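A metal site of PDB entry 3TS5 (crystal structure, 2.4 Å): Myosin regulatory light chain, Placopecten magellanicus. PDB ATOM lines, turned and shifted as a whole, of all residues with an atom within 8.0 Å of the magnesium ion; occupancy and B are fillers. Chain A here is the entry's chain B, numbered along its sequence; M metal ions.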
ATOM      1  N   PHE A  29     -27.563 -19.816  -9.185  1.00  0.00           N
ATOM      2  CA  PHE A  29     -26.888 -20.816  -8.379  1.00  0.00           C
ATOM      3  C   PHE A  29     -25.733 -20.164  -7.606  1.00  0.00           C
ATOM      4  O   PHE A  29     -25.544 -20.391  -6.400  1.00  0.00           O
ATOM      5  CB  PHE A  29     -26.372 -21.960  -9.250  1.00  0.00           C
ATOM      6  CG  PHE A  29     -25.588 -22.979  -8.479  1.00  0.00           C
ATOM      7  CD1 PHE A  29     -26.224 -24.067  -7.887  1.00  0.00           C
ATOM      8  CD2 PHE A  29     -24.215 -22.830  -8.272  1.00  0.00           C
ATOM      9  CE1 PHE A  29     -25.512 -24.992  -7.136  1.00  0.00           C
ATOM     10  CE2 PHE A  29     -23.501 -23.756  -7.531  1.00  0.00           C
ATOM     11  CZ  PHE A  29     -24.160 -24.840  -6.966  1.00  0.00           C
ATOM     12  N   ILE A  32     -26.898 -18.029  -4.614  1.00  0.00           N
ATOM     13  CA  ILE A  32     -27.438 -18.810  -3.508  1.00  0.00           C
ATOM     14  C   ILE A  32     -26.325 -19.531  -2.763  1.00  0.00           C
ATOM     15  O   ILE A  32     -26.387 -19.684  -1.547  1.00  0.00           O
ATOM     16  CB  ILE A  32     -28.509 -19.812  -3.979  1.00  0.00           C
ATOM     17  CG1 ILE A  32     -29.705 -19.057  -4.529  1.00  0.00           C
ATOM     18  CG2 ILE A  32     -28.970 -20.678  -2.830  1.00  0.00           C
ATOM     19  CD1 ILE A  32     -30.630 -19.911  -5.322  1.00  0.00           C
ATOM     20  N   ASP A  33     -25.293 -19.961  -3.488  1.00  0.00           N
ATOM     21  CA  ASP A  33     -24.149 -20.596  -2.853  1.00  0.00           C
ATOM     22  C   ASP A  33     -23.234 -19.577  -2.162  1.00  0.00           C
ATOM     23  O   ASP A  33     -22.105 -19.335  -2.593  1.00  0.00           O
ATOM     24  CB  ASP A  33     -23.351 -21.412  -3.876  1.00  0.00           C
ATOM     25  CG  ASP A  33     -22.149 -22.107  -3.265  1.00  0.00           C
ATOM     26  OD1 ASP A  33     -21.229 -22.498  -4.018  1.00  0.00           O
ATOM     27  OD2 ASP A  33     -22.123 -22.265  -2.028  1.00  0.00           O
ATOM     28  N   GLN A  34     -23.734 -18.995  -1.069  1.00  0.00           N
ATOM     29  CA  GLN A  34     -22.973 -18.021  -0.289  1.00  0.00           C
ATOM     30  C   GLN A  34     -21.585 -18.545   0.112  1.00  0.00           C
ATOM     31  O   GLN A  34     -20.659 -17.782   0.322  1.00  0.00           O
ATOM     32  CB  GLN A  34     -23.762 -17.613   0.968  1.00  0.00           C
ATOM     33  CG  GLN A  34     -25.301 -17.591   0.787  1.00  0.00           C
ATOM     34  CD  GLN A  34     -25.842 -16.239   0.286  1.00  0.00           C
ATOM     35  OE1 GLN A  34     -25.077 -15.295  -0.002  1.00  0.00           O
ATOM     36  NE2 GLN A  34     -27.171 -16.131   0.203  1.00  0.00           N
ATOM     37  N   ASN A  35     -21.476 -19.873   0.221  1.00  0.00           N
ATOM     38  CA  ASN A  35     -20.233 -20.575   0.533  1.00  0.00           C
ATOM     39  C   ASN A  35     -19.153 -20.405  -0.523  1.00  0.00           C
ATOM     40  O   ASN A  35     -17.967 -20.539  -0.216  1.00  0.00           O
ATOM     41  CB  ASN A  35     -20.506 -22.091   0.621  1.00  0.00           C
ATOM     42  CG  ASN A  35     -20.891 -22.544   2.008  1.00  0.00           C
ATOM     43  OD1 ASN A  35     -20.939 -21.745   2.942  1.00  0.00           O
ATOM     44  ND2 ASN A  35     -21.187 -23.822   2.143  1.00  0.00           N
ATOM     45  N   ARG A  36     -19.559 -20.181  -1.780  1.00  0.00           N
ATOM     46  CA  ARG A  36     -18.655 -20.274  -2.941  1.00  0.00           C
ATOM     47  C   ARG A  36     -18.100 -21.689  -3.010  1.00  0.00           C
ATOM     48  O   ARG A  36     -17.173 -22.000  -3.776  1.00  0.00           O
ATOM     49  CB  ARG A  36     -17.525 -19.252  -2.867  1.00  0.00           C
ATOM     50  CG  ARG A  36     -18.009 -17.829  -2.576  1.00  0.00           C
ATOM     51  CD  ARG A  36     -16.862 -16.850  -2.517  1.00  0.00           C
ATOM     52  NE  ARG A  36     -17.353 -15.497  -2.286  1.00  0.00           N
ATOM     53  CZ  ARG A  36     -16.593 -14.400  -2.355  1.00  0.00           C
ATOM     54  NH1 ARG A  36     -15.299 -14.501  -2.641  1.00  0.00           N
ATOM     55  NH2 ARG A  36     -17.139 -13.210  -2.141  1.00  0.00           N
ATOM     56  N   ASP A  37     -18.740 -22.544  -2.233  1.00  0.00           N
ATOM     57  CA  ASP A  37     -18.452 -23.964  -2.150  1.00  0.00           C
ATOM     58  C   ASP A  37     -18.627 -24.723  -3.467  1.00  0.00           C
ATOM     59  O   ASP A  37     -17.935 -25.705  -3.707  1.00  0.00           O
ATOM     60  CB  ASP A  37     -19.397 -24.573  -1.105  1.00  0.00           C
ATOM     61  CG  ASP A  37     -18.897 -25.888  -0.575  1.00  0.00           C
ATOM     62  OD1 ASP A  37     -17.719 -26.223  -0.807  1.00  0.00           O
ATOM     63  OD2 ASP A  37     -19.690 -26.594   0.078  1.00  0.00           O
ATOM     64  N   GLY A  38     -19.567 -24.276  -4.304  1.00  0.00           N
ATOM     65  CA  GLY A  38     -19.963 -25.069  -5.467  1.00  0.00           C
ATOM     66  C   GLY A  38     -21.105 -26.029  -5.145  1.00  0.00           C
ATOM     67  O   GLY A  38     -21.478 -26.867  -5.961  1.00  0.00           O
ATOM     68  N   PHE A  39     -21.643 -25.918  -3.930  1.00  0.00           N
ATOM     69  CA  PHE A  39     -22.824 -26.678  -3.521  1.00  0.00           C
ATOM     70  C   PHE A  39     -23.796 -25.741  -2.853  1.00  0.00           C
ATOM     71  O   PHE A  39     -23.405 -24.794  -2.201  1.00  0.00           O
ATOM     72  CB  PHE A  39     -22.454 -27.799  -2.536  1.00  0.00           C
ATOM     73  CG  PHE A  39     -21.592 -28.860  -3.143  1.00  0.00           C
ATOM     74  CD1 PHE A  39     -22.164 -29.887  -3.876  1.00  0.00           C
ATOM     75  CD2 PHE A  39     -20.211 -28.824  -3.002  1.00  0.00           C
ATOM     76  CE1 PHE A  39     -21.364 -30.866  -4.470  1.00  0.00           C
ATOM     77  CE2 PHE A  39     -19.411 -29.794  -3.586  1.00  0.00           C
ATOM     78  CZ  PHE A  39     -19.984 -30.820  -4.319  1.00  0.00           C
ATOM     79  N   ILE A  40     -25.078 -26.006  -3.003  1.00  0.00           N
ATOM     80  CA  ILE A  40     -26.034 -25.325  -2.156  1.00  0.00           C
ATOM     81  C   ILE A  40     -26.468 -26.277  -1.049  1.00  0.00           C
ATOM     82  O   ILE A  40     -27.009 -27.360  -1.309  1.00  0.00           O
ATOM     83  CB  ILE A  40     -27.256 -24.809  -2.939  1.00  0.00           C
ATOM     84  CG1 ILE A  40     -26.814 -23.717  -3.937  1.00  0.00           C
ATOM     85  CG2 ILE A  40     -28.321 -24.271  -1.958  1.00  0.00           C
ATOM     86  CD1 ILE A  40     -27.880 -23.349  -4.955  1.00  0.00           C
ATOM     87  N   ASP A  41     -26.213 -25.876   0.199  1.00  0.00           N
ATOM     88  CA  ASP A  41     -26.729 -26.630   1.351  1.00  0.00           C
ATOM     89  C   ASP A  41     -27.715 -25.812   2.165  1.00  0.00           C
ATOM     90  O   ASP A  41     -28.134 -24.724   1.745  1.00  0.00           O
ATOM     91  CB  ASP A  41     -25.596 -27.162   2.238  1.00  0.00           C
ATOM     92  CG  ASP A  41     -24.846 -26.064   2.979  1.00  0.00           C
ATOM     93  OD1 ASP A  41     -25.197 -24.867   2.869  1.00  0.00           O
ATOM     94  OD2 ASP A  41     -23.868 -26.406   3.687  1.00  0.00           O
ATOM     95  N   ILE A  42     -28.086 -26.328   3.321  1.00  0.00           N
ATOM     96  CA  ILE A  42     -29.175 -25.735   4.099  1.00  0.00           C
ATOM     97  C   ILE A  42     -28.793 -24.351   4.670  1.00  0.00           C
ATOM     98  O   ILE A  42     -29.651 -23.462   4.791  1.00  0.00           O
ATOM     99  CB  ILE A  42     -29.675 -26.706   5.202  1.00  0.00           C
ATOM    100  CG1 ILE A  42     -30.770 -26.051   6.047  1.00  0.00           C
ATOM    101  CG2 ILE A  42     -28.505 -27.193   6.054  1.00  0.00           C
ATOM    102  CD1 ILE A  42     -31.976 -26.919   6.269  1.00  0.00           C
ATOM    103  N   ASN A  43     -27.515 -24.176   4.986  1.00  0.00           N
ATOM    104  CA  ASN A  43     -27.019 -22.892   5.444  1.00  0.00           C
ATOM    105  C   ASN A  43     -27.068 -21.837   4.341  1.00  0.00           C
ATOM    106  O   ASN A  43     -27.423 -20.680   4.602  1.00  0.00           O
ATOM    107  CB  ASN A  43     -25.576 -23.030   5.977  1.00  0.00           C
ATOM    108  CG  ASN A  43     -25.423 -24.153   6.994  1.00  0.00           C
ATOM    109  OD1 ASN A  43     -26.313 -24.407   7.811  1.00  0.00           O
ATOM    110  ND2 ASN A  43     -24.284 -24.837   6.931  1.00  0.00           N
ATOM    111  N   ASP A  44     -26.701 -22.223   3.117  1.00  0.00           N
ATOM    112  CA  ASP A  44     -26.808 -21.331   1.966  1.00  0.00           C
ATOM    113  C   ASP A  44     -28.237 -20.871   1.774  1.00  0.00           C
ATOM    114  O   ASP A  44     -28.508 -19.677   1.549  1.00  0.00           O
ATOM    115  CB  ASP A  44     -26.326 -22.021   0.699  1.00  0.00           C
ATOM    116  CG  ASP A  44     -24.823 -22.179   0.671  1.00  0.00           C
ATOM    117  OD1 ASP A  44     -24.119 -21.245   1.140  1.00  0.00           O
ATOM    118  OD2 ASP A  44     -24.334 -23.216   0.200  1.00  0.00           O
ATOM    119  N   LEU A  45     -29.150 -21.830   1.883  1.00  0.00           N
ATOM    120  CA  LEU A  45     -30.581 -21.583   1.719  1.00  0.00           C
ATOM    121  C   LEU A  45     -31.134 -20.657   2.806  1.00  0.00           C
ATOM    122  O   LEU A  45     -31.850 -19.691   2.485  1.00  0.00           O
ATOM    123  CB  LEU A  45     -31.336 -22.924   1.727  1.00  0.00           C
ATOM    124  CG  LEU A  45     -32.203 -23.291   0.528  1.00  0.00           C
ATOM    125  CD1 LEU A  45     -31.592 -22.806  -0.776  1.00  0.00           C
ATOM    126  CD2 LEU A  45     -32.456 -24.800   0.497  1.00  0.00           C
ATOM    127  N   LEU A  72     -26.165 -30.760  -3.926  1.00  0.00           N
ATOM    128  CA  LEU A  72     -26.628 -29.745  -4.858  1.00  0.00           C
ATOM    129  C   LEU A  72     -25.518 -28.961  -5.561  1.00  0.00           C
ATOM    130  O   LEU A  72     -25.316 -27.789  -5.302  1.00  0.00           O
ATOM    131  CB  LEU A  72     -27.610 -28.795  -4.182  1.00  0.00           C
ATOM    132  CG  LEU A  72     -28.961 -28.653  -4.878  1.00  0.00           C
ATOM    133  CD1 LEU A  72     -29.805 -27.595  -4.174  1.00  0.00           C
ATOM    134  CD2 LEU A  72     -28.757 -28.280  -6.346  1.00  0.00           C
HETATM  135 MG    MG M   1     -22.305 -23.951  -0.421  1.00  0.00          MG
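Residues that only touch the magnesium ion: Asp 37 (3.1 Å). Within 4 Å of the magnesium ion: Asp 33, Asn 35, Asp 37, Phe 39 and Asp 44. The nearest printed residue that does not touch the magnesium ion is Ile 40 (4.3 Å).
OD1 of Asp 44 is in hydrogen-bond range of N of Gln 34, 3.2 Å away. The backbone NH (N) of Asp 44 sits at hydrogen-bond distance from the side-chain carboxylate (OD1) of Asp 41, at 3.1 Å. OD1 of Asp 44 lies within hydrogen-bond range of N of Asn 35. OD1 of Asp 33 is in hydrogen-bond range of N of Asp 37. OD2 of Asp 33 sits close to N of Arg 36, at 3.3 Å. The backbone NH (N) of Asn 35 lies close to the side-chain carboxylate (OD2) of Asp 33, 3.3 Å away. OD1 of Asp 33 sits at hydrogen-bond distance from N of Gly 38, at 2.5 Å.
OD2 of Asp 44 binds the magnesium ion, 2.2 Å away. O of Phe 39 binds the magnesium ion, at 2.3 Å. The magnesium ion is bound by OD2 of Asp 33. Slightly farther from the magnesium ion lies the side-chain amide nitrogen (ND2) of Asn 35 (2.8 Å).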
